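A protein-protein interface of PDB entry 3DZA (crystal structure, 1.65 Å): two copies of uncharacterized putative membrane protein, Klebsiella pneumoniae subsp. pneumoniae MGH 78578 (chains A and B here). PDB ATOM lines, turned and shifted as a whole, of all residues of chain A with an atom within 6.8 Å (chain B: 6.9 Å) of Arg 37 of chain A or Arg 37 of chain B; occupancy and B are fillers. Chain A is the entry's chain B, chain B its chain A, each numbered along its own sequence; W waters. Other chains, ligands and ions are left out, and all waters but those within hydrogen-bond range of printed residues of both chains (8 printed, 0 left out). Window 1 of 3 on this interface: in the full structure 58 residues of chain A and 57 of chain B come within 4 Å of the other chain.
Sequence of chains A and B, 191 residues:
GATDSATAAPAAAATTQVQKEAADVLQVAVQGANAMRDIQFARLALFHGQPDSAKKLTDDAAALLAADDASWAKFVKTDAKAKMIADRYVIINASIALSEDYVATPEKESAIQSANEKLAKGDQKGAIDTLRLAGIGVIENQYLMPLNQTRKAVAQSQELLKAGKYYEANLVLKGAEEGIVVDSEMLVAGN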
ATOM      1  N   GLN A  19     -11.889 -21.359   5.725  1.00  0.00           N
ATOM      2  CA  GLN A  19     -12.585 -20.999   4.485  1.00  0.00           C
ATOM      3  C   GLN A  19     -14.010 -21.565   4.405  1.00  0.00           C
ATOM      4  O   GLN A  19     -14.936 -20.836   3.974  1.00  0.00           O
ATOM      5  CB  GLN A  19     -11.775 -21.428   3.265  1.00  0.00           C
ATOM      6  CG  GLN A  19     -10.500 -20.653   3.055  1.00  0.00           C
ATOM      7  CD  GLN A  19      -9.850 -20.933   1.707  1.00  0.00           C
ATOM      8  OE1 GLN A  19     -10.402 -21.692   0.908  1.00  0.00           O
ATOM      9  NE2 GLN A  19      -8.696 -20.331   1.453  1.00  0.00           N
ATOM     10  N   VAL A  30     -17.484 -22.669  -1.513  1.00  0.00           N
ATOM     11  CA  VAL A  30     -16.026 -22.811  -1.707  1.00  0.00           C
ATOM     12  C   VAL A  30     -15.637 -24.173  -2.290  1.00  0.00           C
ATOM     13  O   VAL A  30     -14.683 -24.280  -3.058  1.00  0.00           O
ATOM     14  CB  VAL A  30     -15.207 -22.476  -0.439  1.00  0.00           C
ATOM     15  CG1 VAL A  30     -15.329 -23.582   0.627  1.00  0.00           C
ATOM     16  CG2 VAL A  30     -13.748 -22.216  -0.823  1.00  0.00           C
ATOM     17  N   GLY A  32     -17.026 -25.567  -4.746  1.00  0.00           N
ATOM     18  CA  GLY A  32     -17.051 -25.238  -6.163  1.00  0.00           C
ATOM     19  C   GLY A  32     -15.809 -24.494  -6.639  1.00  0.00           C
ATOM     20  O   GLY A  32     -15.222 -24.830  -7.682  1.00  0.00           O
ATOM     21  N   ALA A  33     -15.409 -23.477  -5.881  1.00  0.00           N
ATOM     22  CA  ALA A  33     -14.161 -22.749  -6.177  1.00  0.00           C
ATOM     23  C   ALA A  33     -12.977 -23.739  -6.216  1.00  0.00           C
ATOM     24  O   ALA A  33     -12.100 -23.688  -7.101  1.00  0.00           O
ATOM     25  CB  ALA A  33     -13.937 -21.621  -5.130  1.00  0.00           C
ATOM     26  N   ASN A  34     -12.968 -24.671  -5.276  1.00  0.00           N
ATOM     27  CA  ASN A  34     -11.896 -25.661  -5.188  1.00  0.00           C
ATOM     28  C   ASN A  34     -11.873 -26.613  -6.395  1.00  0.00           C
ATOM     29  O   ASN A  34     -10.812 -26.940  -6.942  1.00  0.00           O
ATOM     30  CB  ASN A  34     -12.025 -26.448  -3.856  1.00  0.00           C
ATOM     31  CG  ASN A  34     -11.649 -25.627  -2.637  1.00  0.00           C
ATOM     32  OD1 ASN A  34     -10.940 -24.634  -2.737  1.00  0.00           O
ATOM     33  ND2 ASN A  34     -12.128 -26.049  -1.462  1.00  0.00           N
ATOM     34  N   ALA A  35     -13.057 -27.043  -6.822  1.00  0.00           N
ATOM     35  CA  ALA A  35     -13.179 -27.867  -8.021  1.00  0.00           C
ATOM     36  C   ALA A  35     -12.662 -27.123  -9.230  1.00  0.00           C
ATOM     37  O   ALA A  35     -11.947 -27.680 -10.076  1.00  0.00           O
ATOM     38  CB  ALA A  35     -14.660 -28.315  -8.234  1.00  0.00           C
ATOM     39  N   MET A  36     -13.001 -25.840  -9.333  1.00  0.00           N
ATOM     40  CA  MET A  36     -12.552 -25.068 -10.472  1.00  0.00           C
ATOM     41  C   MET A  36     -11.042 -24.850 -10.440  1.00  0.00           C
ATOM     42  O   MET A  36     -10.417 -24.852 -11.495  1.00  0.00           O
ATOM     43  CB  MET A  36     -13.289 -23.735 -10.575  1.00  0.00           C
ATOM     44  CG  MET A  36     -14.798 -23.840 -10.749  1.00  0.00           C
ATOM     45  SD  MET A  36     -15.400 -25.103 -12.137  1.00  0.00           S
ATOM     46  CE  MET A  36     -14.576 -24.323 -13.673  1.00  0.00           C
ATOM     47  N   ARG A  37     -10.459 -24.680  -9.250  1.00  0.00           N
ATOM     48  CA  ARG A  37      -9.012 -24.531  -9.152  1.00  0.00           C
ATOM     49  C   ARG A  37      -8.321 -25.847  -9.528  1.00  0.00           C
ATOM     50  O   ARG A  37      -7.296 -25.828 -10.200  1.00  0.00           O
ATOM     51  CB  ARG A  37      -8.542 -24.040  -7.778  1.00  0.00           C
ATOM     52  CG  ARG A  37      -7.068 -23.747  -7.745  1.00  0.00           C
ATOM     53  CD  ARG A  37      -6.680 -22.916  -6.528  1.00  0.00           C
ATOM     54  NE  ARG A  37      -6.970 -21.502  -6.713  1.00  0.00           N
ATOM     55  CZ  ARG A  37      -6.916 -20.592  -5.732  1.00  0.00           C
ATOM     56  NH1 ARG A  37      -6.653 -20.939  -4.465  1.00  0.00           N
ATOM     57  NH2 ARG A  37      -7.175 -19.320  -6.007  1.00  0.00           N
ATOM     58  N   ASP A  38      -8.864 -26.980  -9.092  1.00  0.00           N
ATOM     59  CA  ASP A  38      -8.407 -28.299  -9.570  1.00  0.00           C
ATOM     60  C   ASP A  38      -8.376 -28.365 -11.120  1.00  0.00           C
ATOM     61  O   ASP A  38      -7.373 -28.839 -11.689  1.00  0.00           O
ATOM     62  CB  ASP A  38      -9.330 -29.431  -9.074  1.00  0.00           C
ATOM     63  CG  ASP A  38      -9.219 -29.769  -7.597  1.00  0.00           C
ATOM     64  OD1 ASP A  38      -8.258 -29.362  -6.898  1.00  0.00           O
ATOM     65  OD2 ASP A  38     -10.130 -30.546  -7.171  1.00  0.00           O
ATOM     66  N   ILE A  39      -9.456 -27.914 -11.780  1.00  0.00           N
ATOM     67  CA  ILE A  39      -9.608 -27.917 -13.233  1.00  0.00           C
ATOM     68  C   ILE A  39      -8.520 -27.026 -13.882  1.00  0.00           C
ATOM     69  O   ILE A  39      -7.831 -27.443 -14.816  1.00  0.00           O
ATOM     70  CB  ILE A  39     -11.057 -27.455 -13.662  1.00  0.00           C
ATOM     71  CG1 ILE A  39     -12.083 -28.553 -13.377  1.00  0.00           C
ATOM     72  CG2 ILE A  39     -11.084 -26.985 -15.109  1.00  0.00           C
ATOM     73  CD1 ILE A  39     -13.525 -28.076 -13.469  1.00  0.00           C
ATOM     74  N   GLN A  40      -8.359 -25.821 -13.342  1.00  0.00           N
ATOM     75  CA  GLN A  40      -7.307 -24.915 -13.733  1.00  0.00           C
ATOM     76  C   GLN A  40      -5.922 -25.564 -13.623  1.00  0.00           C
ATOM     77  O   GLN A  40      -5.109 -25.486 -14.553  1.00  0.00           O
ATOM     78  CB  GLN A  40      -7.357 -23.692 -12.807  1.00  0.00           C
ATOM     79  CG  GLN A  40      -6.270 -22.654 -13.015  1.00  0.00           C
ATOM     80  CD  GLN A  40      -6.132 -21.759 -11.787  1.00  0.00           C
ATOM     81  OE1 GLN A  40      -7.092 -21.581 -11.023  1.00  0.00           O
ATOM     82  NE2 GLN A  40      -4.942 -21.194 -11.587  1.00  0.00           N
ATOM     83  N   PHE A  41      -5.612 -26.162 -12.487  1.00  0.00           N
ATOM     84  CA  PHE A  41      -4.323 -26.790 -12.332  1.00  0.00           C
ATOM     85  C   PHE A  41      -4.165 -28.011 -13.242  1.00  0.00           C
ATOM     86  O   PHE A  41      -3.033 -28.385 -13.628  1.00  0.00           O
ATOM     87  CB  PHE A  41      -4.079 -27.210 -10.897  1.00  0.00           C
ATOM     88  CG  PHE A  41      -3.793 -26.076  -9.924  1.00  0.00           C
ATOM     89  CD1 PHE A  41      -3.590 -24.738 -10.302  1.00  0.00           C
ATOM     90  CD2 PHE A  41      -3.660 -26.394  -8.590  1.00  0.00           C
ATOM     91  CE1 PHE A  41      -3.299 -23.772  -9.356  1.00  0.00           C
ATOM     92  CE2 PHE A  41      -3.374 -25.417  -7.642  1.00  0.00           C
ATOM     93  CZ  PHE A  41      -3.192 -24.113  -8.033  1.00  0.00           C
ATOM     94  N   ALA A  42      -5.277 -28.679 -13.532  1.00  0.00           N
ATOM     95  CA  ALA A  42      -5.218 -29.875 -14.408  1.00  0.00           C
ATOM     96  C   ALA A  42      -4.776 -29.452 -15.803  1.00  0.00           C
ATOM     97  O   ALA A  42      -3.948 -30.123 -16.445  1.00  0.00           O
ATOM     98  CB  ALA A  42      -6.595 -30.597 -14.491  1.00  0.00           C
ATOM     99  N   LEU A  57      -5.973 -34.398 -10.300  1.00  0.00           N
ATOM    100  CA  LEU A  57      -6.699 -33.132 -10.125  1.00  0.00           C
ATOM    101  C   LEU A  57      -8.125 -33.210 -10.673  1.00  0.00           C
ATOM    102  O   LEU A  57      -9.109 -32.727 -10.051  1.00  0.00           O
ATOM    103  CB  LEU A  57      -5.927 -31.985 -10.821  1.00  0.00           C
ATOM    104  CG  LEU A  57      -4.621 -31.555 -10.143  1.00  0.00           C
ATOM    105  CD1 LEU A  57      -3.628 -30.927 -11.151  1.00  0.00           C
ATOM    106  CD2 LEU A  57      -4.884 -30.598  -8.989  1.00  0.00           C
ATOM    107  N   ILE A  92     -20.242 -20.031  -6.460  1.00  0.00           N
ATOM    108  CA  ILE A  92     -19.055 -20.782  -6.025  1.00  0.00           C
ATOM    109  C   ILE A  92     -17.916 -19.862  -5.591  1.00  0.00           C
ATOM    110  O   ILE A  92     -16.923 -20.311  -5.033  1.00  0.00           O
ATOM    111  CB  ILE A  92     -18.566 -21.759  -7.129  1.00  0.00           C
ATOM    112  CG1 ILE A  92     -18.152 -20.982  -8.393  1.00  0.00           C
ATOM    113  CG2 ILE A  92     -19.628 -22.844  -7.420  1.00  0.00           C
ATOM    114  CD1 ILE A  92     -17.182 -21.782  -9.284  1.00  0.00           C
ATOM    115  N   ASN A  93     -18.035 -18.574  -5.876  1.00  0.00           N
ATOM    116  CA  ASN A  93     -16.992 -17.610  -5.515  1.00  0.00           C
ATOM    117  C   ASN A  93     -17.630 -16.223  -5.591  1.00  0.00           C
ATOM    118  O   ASN A  93     -18.654 -16.031  -6.252  1.00  0.00           O
ATOM    119  CB  ASN A  93     -15.763 -17.772  -6.457  1.00  0.00           C
ATOM    120  CG  ASN A  93     -14.445 -17.402  -5.814  1.00  0.00           C
ATOM    121  OD1 ASN A  93     -14.405 -16.751  -4.759  1.00  0.00           O
ATOM    122  ND2 ASN A  93     -13.337 -17.828  -6.454  1.00  0.00           N
ATOM    123  N   GLU A 177     -14.522 -23.966 -17.652  1.00  0.00           N
ATOM    124  CA  GLU A 177     -14.155 -22.680 -17.104  1.00  0.00           C
ATOM    125  C   GLU A 177     -14.928 -21.512 -17.747  1.00  0.00           C
ATOM    126  O   GLU A 177     -15.329 -20.549 -17.058  1.00  0.00           O
ATOM    127  CB  GLU A 177     -12.656 -22.472 -17.272  1.00  0.00           C
ATOM    128  CG  GLU A 177     -11.793 -23.454 -16.532  1.00  0.00           C
ATOM    129  CD  GLU A 177     -10.326 -23.242 -16.732  1.00  0.00           C
ATOM    130  OE1 GLU A 177      -9.918 -22.990 -17.883  1.00  0.00           O
ATOM    131  OE2 GLU A 177      -9.574 -23.255 -15.726  1.00  0.00           O
ATOM    132  N   GLN B  19      -3.816 -30.783  -4.489  1.00  0.00           N
ATOM    133  CA  GLN B  19      -3.321 -29.480  -4.978  1.00  0.00           C
ATOM    134  C   GLN B  19      -1.870 -29.249  -4.594  1.00  0.00           C
ATOM    135  O   GLN B  19      -1.113 -28.721  -5.370  1.00  0.00           O
ATOM    136  CB  GLN B  19      -4.202 -28.339  -4.473  1.00  0.00           C
ATOM    137  CG  GLN B  19      -5.557 -28.319  -5.141  1.00  0.00           C
ATOM    138  CD  GLN B  19      -6.331 -27.066  -4.790  1.00  0.00           C
ATOM    139  OE1 GLN B  19      -5.832 -26.237  -4.032  1.00  0.00           O
ATOM    140  NE2 GLN B  19      -7.565 -26.924  -5.331  1.00  0.00           N
ATOM    141  N   VAL B  30       0.894 -22.912  -3.926  1.00  0.00           N
ATOM    142  CA  VAL B  30      -0.542 -22.872  -3.690  1.00  0.00           C
ATOM    143  C   VAL B  30      -0.855 -22.288  -2.312  1.00  0.00           C
ATOM    144  O   VAL B  30      -1.911 -21.693  -2.118  1.00  0.00           O
ATOM    145  CB  VAL B  30      -1.216 -24.254  -3.918  1.00  0.00           C
ATOM    146  CG1 VAL B  30      -0.709 -25.322  -2.839  1.00  0.00           C
ATOM    147  CG2 VAL B  30      -2.779 -24.108  -4.010  1.00  0.00           C
ATOM    148  N   GLY B  32       0.401 -19.650  -1.162  1.00  0.00           N
ATOM    149  CA  GLY B  32       0.163 -18.262  -1.467  1.00  0.00           C
ATOM    150  C   GLY B  32      -1.237 -17.971  -2.043  1.00  0.00           C
ATOM    151  O   GLY B  32      -1.925 -17.022  -1.599  1.00  0.00           O
ATOM    152  N   ALA B  33      -1.679 -18.783  -3.001  1.00  0.00           N
ATOM    153  CA  ALA B  33      -3.048 -18.656  -3.511  1.00  0.00           C
ATOM    154  C   ALA B  33      -4.047 -18.781  -2.372  1.00  0.00           C
ATOM    155  O   ALA B  33      -5.045 -18.049  -2.326  1.00  0.00           O
ATOM    156  CB  ALA B  33      -3.311 -19.685  -4.610  1.00  0.00           C
ATOM    157  N   ASN B  34      -3.805 -19.727  -1.469  1.00  0.00           N
ATOM    158  CA  ASN B  34      -4.681 -19.909  -0.320  1.00  0.00           C
ATOM    159  C   ASN B  34      -4.738 -18.676   0.585  1.00  0.00           C
ATOM    160  O   ASN B  34      -5.840 -18.249   1.025  1.00  0.00           O
ATOM    161  CB  ASN B  34      -4.264 -21.155   0.430  1.00  0.00           C
ATOM    162  CG  ASN B  34      -4.605 -22.435  -0.357  1.00  0.00           C
ATOM    163  OD1 ASN B  34      -5.439 -22.392  -1.237  1.00  0.00           O
ATOM    164  ND2 ASN B  34      -3.962 -23.569  -0.015  1.00  0.00           N
ATOM    165  N   ALA B  35      -3.569 -18.101   0.865  1.00  0.00           N
ATOM    166  CA  ALA B  35      -3.476 -16.852   1.632  1.00  0.00           C
ATOM    167  C   ALA B  35      -4.262 -15.729   0.957  1.00  0.00           C
ATOM    168  O   ALA B  35      -4.964 -14.967   1.610  1.00  0.00           O
ATOM    169  CB  ALA B  35      -2.019 -16.462   1.855  1.00  0.00           C
ATOM    170  N   MET B  36      -4.170 -15.636  -0.361  1.00  0.00           N
ATOM    171  CA  MET B  36      -4.885 -14.566  -1.095  1.00  0.00           C
ATOM    172  C   MET B  36      -6.383 -14.798  -1.102  1.00  0.00           C
ATOM    173  O   MET B  36      -7.161 -13.835  -1.024  1.00  0.00           O
ATOM    174  CB  MET B  36      -4.378 -14.413  -2.534  1.00  0.00           C
ATOM    175  CG  MET B  36      -2.922 -13.953  -2.690  1.00  0.00           C
ATOM    176  SD  MET B  36      -2.269 -12.580  -1.411  1.00  0.00           S
ATOM    177  CE  MET B  36      -3.452 -11.228  -2.005  1.00  0.00           C
ATOM    178  N   ARG B  37      -6.810 -16.054  -1.188  1.00  0.00           N
ATOM    179  CA  ARG B  37      -8.257 -16.335  -1.117  1.00  0.00           C
ATOM    180  C   ARG B  37      -8.775 -16.011   0.297  1.00  0.00           C
ATOM    181  O   ARG B  37      -9.879 -15.471   0.465  1.00  0.00           O
ATOM    182  CB  ARG B  37      -8.578 -17.787  -1.502  1.00  0.00           C
ATOM    183  CG  ARG B  37     -10.099 -18.044  -1.737  1.00  0.00           C
ATOM    184  CD  ARG B  37     -10.381 -19.377  -2.516  1.00  0.00           C
ATOM    185  NE  ARG B  37     -10.363 -19.202  -3.975  1.00  0.00           N
ATOM    186  CZ  ARG B  37     -10.341 -20.187  -4.894  1.00  0.00           C
ATOM    187  NH1 ARG B  37     -10.289 -21.489  -4.560  1.00  0.00           N
ATOM    188  NH2 ARG B  37     -10.339 -19.873  -6.194  1.00  0.00           N
ATOM    189  N   ASP B  38      -7.980 -16.318   1.314  1.00  0.00           N
ATOM    190  CA  ASP B  38      -8.329 -15.926   2.681  1.00  0.00           C
ATOM    191  C   ASP B  38      -8.600 -14.425   2.730  1.00  0.00           C
ATOM    192  O   ASP B  38      -9.592 -13.944   3.313  1.00  0.00           O
ATOM    193  CB  ASP B  38      -7.238 -16.231   3.708  1.00  0.00           C
ATOM    194  CG  ASP B  38      -7.097 -17.705   4.067  1.00  0.00           C
ATOM    195  OD1 ASP B  38      -8.019 -18.485   3.788  1.00  0.00           O
ATOM    196  OD2 ASP B  38      -6.017 -18.061   4.663  1.00  0.00           O
ATOM    197  N   ILE B  39      -7.668 -13.659   2.151  1.00  0.00           N
ATOM    198  CA  ILE B  39      -7.749 -12.197   2.104  1.00  0.00           C
ATOM    199  C   ILE B  39      -9.041 -11.715   1.379  1.00  0.00           C
ATOM    200  O   ILE B  39      -9.799 -10.851   1.872  1.00  0.00           O
ATOM    201  CB  ILE B  39      -6.463 -11.586   1.473  1.00  0.00           C
ATOM    202  CG1 ILE B  39      -5.306 -11.662   2.469  1.00  0.00           C
ATOM    203  CG2 ILE B  39      -6.737 -10.134   1.056  1.00  0.00           C
ATOM    204  CD1 ILE B  39      -3.915 -11.388   1.897  1.00  0.00           C
ATOM    205  N   GLN B  40      -9.279 -12.310   0.219  1.00  0.00           N
ATOM    206  CA  GLN B  40     -10.488 -12.074  -0.572  1.00  0.00           C
ATOM    207  C   GLN B  40     -11.756 -12.288   0.254  1.00  0.00           C
ATOM    208  O   GLN B  40     -12.657 -11.425   0.310  1.00  0.00           O
ATOM    209  CB  GLN B  40     -10.495 -13.011  -1.762  1.00  0.00           C
ATOM    210  CG  GLN B  40     -11.690 -12.885  -2.682  1.00  0.00           C
ATOM    211  CD  GLN B  40     -11.801 -14.119  -3.546  1.00  0.00           C
ATOM    212  OE1 GLN B  40     -10.793 -14.802  -3.805  1.00  0.00           O
ATOM    213  NE2 GLN B  40     -13.016 -14.479  -3.907  1.00  0.00           N
ATOM    214  N   PHE B  41     -11.838 -13.451   0.895  1.00  0.00           N
ATOM    215  CA  PHE B  41     -12.997 -13.788   1.697  1.00  0.00           C
ATOM    216  C   PHE B  41     -13.096 -12.876   2.929  1.00  0.00           C
ATOM    217  O   PHE B  41     -14.197 -12.568   3.360  1.00  0.00           O
ATOM    218  CB  PHE B  41     -12.911 -15.252   2.129  1.00  0.00           C
ATOM    219  CG  PHE B  41     -13.262 -16.279   1.051  1.00  0.00           C
ATOM    220  CD1 PHE B  41     -13.570 -15.938  -0.268  1.00  0.00           C
ATOM    221  CD2 PHE B  41     -13.307 -17.645   1.413  1.00  0.00           C
ATOM    222  CE1 PHE B  41     -13.870 -16.949  -1.234  1.00  0.00           C
ATOM    223  CE2 PHE B  41     -13.629 -18.627   0.474  1.00  0.00           C
ATOM    224  CZ  PHE B  41     -13.929 -18.274  -0.845  1.00  0.00           C
ATOM    225  N   ALA B  42     -11.970 -12.447   3.498  1.00  0.00           N
ATOM    226  CA  ALA B  42     -11.977 -11.513   4.651  1.00  0.00           C
ATOM    227  C   ALA B  42     -12.674 -10.195   4.259  1.00  0.00           C
ATOM    228  O   ALA B  42     -13.529  -9.681   5.000  1.00  0.00           O
ATOM    229  CB  ALA B  42     -10.541 -11.252   5.226  1.00  0.00           C
ATOM    230  N   ARG B  43     -12.328  -9.648   3.087  1.00  0.00           N
ATOM    231  CA  ARG B  43     -12.973  -8.443   2.651  1.00  0.00           C
ATOM    232  C   ARG B  43     -14.501  -8.672   2.454  1.00  0.00           C
ATOM    233  O   ARG B  43     -15.337  -7.828   2.839  1.00  0.00           O
ATOM    234  CB  ARG B  43     -12.330  -7.908   1.361  1.00  0.00           C
ATOM    235  CG  ARG B  43     -10.845  -7.516   1.475  1.00  0.00           C
ATOM    236  CD  ARG B  43     -10.319  -6.947   0.172  1.00  0.00           C
ATOM    237  NE  ARG B  43     -11.029  -5.728  -0.172  1.00  0.00           N
ATOM    238  CZ  ARG B  43     -11.399  -5.352  -1.397  1.00  0.00           C
ATOM    239  NH1 ARG B  43     -11.031  -6.057  -2.472  1.00  0.00           N
ATOM    240  NH2 ARG B  43     -12.061  -4.200  -1.554  1.00  0.00           N
ATOM    241  N   LEU B  57     -10.093 -15.315   9.011  1.00  0.00           N
ATOM    242  CA  LEU B  57      -9.527 -15.438   7.648  1.00  0.00           C
ATOM    243  C   LEU B  57      -8.182 -14.716   7.549  1.00  0.00           C
ATOM    244  O   LEU B  57      -7.203 -15.246   6.972  1.00  0.00           O
ATOM    245  CB  LEU B  57     -10.520 -14.869   6.633  1.00  0.00           C
ATOM    246  CG  LEU B  57     -11.726 -15.806   6.384  1.00  0.00           C
ATOM    247  CD1 LEU B  57     -12.960 -14.996   5.902  1.00  0.00           C
ATOM    248  CD2 LEU B  57     -11.328 -16.968   5.449  1.00  0.00           C
ATOM    249  N   ILE B  92       2.522 -17.624  -7.023  1.00  0.00           N
ATOM    250  CA  ILE B  92       1.488 -18.200  -6.151  1.00  0.00           C
ATOM    251  C   ILE B  92       0.318 -18.825  -6.929  1.00  0.00           C
ATOM    252  O   ILE B  92      -0.496 -19.554  -6.361  1.00  0.00           O
ATOM    253  CB  ILE B  92       0.944 -17.193  -5.128  1.00  0.00           C
ATOM    254  CG1 ILE B  92       0.329 -15.955  -5.820  1.00  0.00           C
ATOM    255  CG2 ILE B  92       2.085 -16.791  -4.149  1.00  0.00           C
ATOM    256  CD1 ILE B  92      -0.673 -15.176  -4.983  1.00  0.00           C
ATOM    257  N   ASN B  93       0.237 -18.518  -8.207  1.00  0.00           N
ATOM    258  CA  ASN B  93      -0.825 -19.044  -9.030  1.00  0.00           C
ATOM    259  C   ASN B  93      -0.395 -18.947 -10.495  1.00  0.00           C
ATOM    260  O   ASN B  93       0.441 -18.151 -10.854  1.00  0.00           O
ATOM    261  CB  ASN B  93      -2.126 -18.256  -8.795  1.00  0.00           C
ATOM    262  CG  ASN B  93      -3.392 -19.087  -9.014  1.00  0.00           C
ATOM    263  OD1 ASN B  93      -3.365 -20.120  -9.640  1.00  0.00           O
ATOM    264  ND2 ASN B  93      -4.512 -18.614  -8.465  1.00  0.00           N
ATOM    265  N   GLU B 177      -4.110  -7.263  -2.491  1.00  0.00           N
ATOM    266  CA  GLU B 177      -4.542  -7.938  -3.711  1.00  0.00           C
ATOM    267  C   GLU B 177      -3.962  -7.229  -4.923  1.00  0.00           C
ATOM    268  O   GLU B 177      -3.527  -7.867  -5.898  1.00  0.00           O
ATOM    269  CB  GLU B 177      -6.055  -7.957  -3.787  1.00  0.00           C
ATOM    270  CG  GLU B 177      -6.654  -8.743  -2.631  1.00  0.00           C
ATOM    271  CD  GLU B 177      -8.174  -8.755  -2.667  1.00  0.00           C
ATOM    272  OE1 GLU B 177      -8.793  -7.676  -2.814  1.00  0.00           O
ATOM    273  OE2 GLU B 177      -8.723  -9.867  -2.578  1.00  0.00           O
HETATM  274  O   HOH W   1      -7.809 -21.094  -1.429  1.00  0.00           O
HETATM  275  O   HOH W   2      -8.800 -24.191  -4.361  1.00  0.00           O
HETATM  276  O   HOH W   3     -10.241 -22.181  -1.789  1.00  0.00           O
HETATM  277  O   HOH W   4      -7.193 -19.765  -9.119  1.00  0.00           O
HETATM  278  O   HOH W   5     -11.320 -21.422  -8.424  1.00  0.00           O
HETATM  279  O   HOH W   6      -6.184 -23.561  -3.538  1.00  0.00           O
HETATM  280  O   HOH W   7      -6.331 -16.850  -4.625  1.00  0.00           O
HETATM  281  O   HOH W   8     -10.624 -16.708  -5.599  1.00  0.00           O
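Water W8 lies within hydrogen-bond range of the side-chain amide oxygen of Gln 40 of chain B (2.6 Å), the guanidinium group of Arg 37 of chain B (3.0 Å) and the side-chain amide nitrogen of Asn 93 of chain A (3.1 Å).
Water W1 lies within hydrogen-bond range of the side-chain amide oxygen of Asn 34 of chain B (2.7 Å), the side-chain amide nitrogen of Gln 19 of chain A (3.1 Å) and the guanidinium group of Arg 37 of chain A (3.3 Å).
Water W3 lies within hydrogen-bond range of the side-chain amide oxygen of Asn 34 of chain A (2.7 Å), the side-chain amide oxygen of Gln 19 of chain A (2.7 Å) and the guanidinium group of Arg 37 of chain B (2.9 Å).
Water W2 lies within hydrogen-bond range of OD1 of Asn 34 of chain A (2.7 Å), NH1 of Arg 37 of chain B (3.1 Å) and NE2 of Gln 19 of chain B (3.2 Å).
Water W5 lies within hydrogen-bond range of the backbone carbonyl oxygen of Ala 33 of chain A (2.7 Å), the guanidinium group of Arg 37 of chain B (2.9 Å) and the backbone NH of Arg 37 of chain A (3.5 Å).
Water W7 lies within hydrogen-bond range of O of Ala 33 of chain B and NH2 of Arg 37 of chain A.
Gln 19 of chain A touches Asp 38 of chain B, and with the chains exchanged Asp 38 of chain A touches Gln 19 of chain B.
Arg 37 of chain A touches its own counterpart, Arg 37 of chain B.
Arg 37 of chain A touches Asn 93 of chain B, and with the chains exchanged Asn 93 of chain A touches Arg 37 of chain B.
Phe 41 of chain A touches Asn 93 of chain B, and with the chains exchanged Asn 93 of chain A touches Phe 41 of chain B.
Of the 19 pairs that touch across the chains among the printed residues, 19 have their exchanged pair printed and touching as well.
O of Asn 34 of chain B touches NE2 of Gln 19 of chain A, at 3.6 Å.
Phe 41 of chain B touches Val 30 of chain A.
Arg 37 of chain B touches Ala 33 of chain A (NH1 to CB, 3.7 Å).
O of Asn 34 of chain A touches NE2 of Gln 19 of chain B (3.6 Å).
Asn 34 of chain A touches Arg 37 of chain B (OD1 to NH1, 3.7 Å).
OD1 of Asn 34 of chain B touches NH1 of Arg 37 of chain A (3.7 Å).
Arg 37 of chain A touches Asn 93 of chain B.
CE2 of Phe 41 of chain A touches CG2 of Val 30 of chain B (3.9 Å).
ND2 of Asn 93 of chain A touches NH2 of Arg 37 of chain B (3.6 Å).
Phe 41 of chain B touches Asn 93 of chain A.
Hydrophobic or aromatic side chains of chain A that line the printed part of chain B: Val 30, Ala 33 and Phe 41.
Hydrophobic or aromatic side chains of chain B within 4 Å of the printed part of chain A: Val 30, Ala 33 and Phe 41.
Among the printed residues, no Asp or Glu carboxylate lies within 4 Å of a Lys or Arg side-chain nitrogen of the other chain.
Printed residues of chain B within 4 Å of Val 30 of chain A: Phe 41 (3.8 Å).
Arg 37 of chain A touches just these residues of chain B: Gln 19, Ala 33, Asn 34, Arg 37 and Asn 93.
Of the printed residues of chain B, Asn 93 of chain A touches Arg 37, Gln 40 and Phe 41.
Of chain A, only Gln 19, Ala 33, Asn 34, Arg 37 and Asn 93 come within 4 Å of Arg 37 of chain B.
Printed residues of chain A within 4 Å of Phe 41 of chain B: Val 30 and Asn 93.
The nearest residue of chain B that does not touch Arg 37 of chain A is Val 30 of chain B (4.8 Å).
NE2 of Gln 19 of chain B is in hydrogen-bond range of OD1 of Asp 38 of chain A (3.0 Å).
The side-chain amide nitrogen (NE2) of Gln 19 of chain A lies within hydrogen-bond range of the side-chain carboxylate (OD1) of Asp 38 of chain B.
NE2 of Gln 40 of chain B lies within hydrogen-bond range of OD1 of Asn 93 of chain A (2.8 Å).
The side-chain amide nitrogen (NE2) of Gln 40 of chain A lies within hydrogen-bond range of the side-chain amide oxygen (OD1) of Asn 93 of chain B.
The guanidinium group (NH2) of Arg 37 of chain B lies close to the guanidinium group (NH2) of Arg 37 of chain A.
The side-chain amide nitrogen of Asn 34 of chain B sits close to the backbone carbonyl oxygen of Val 30 of chain B (3.5 Å).
ND2 of Asn 34 of chain A lies close to O of Val 30 of chain A (3.5 Å).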
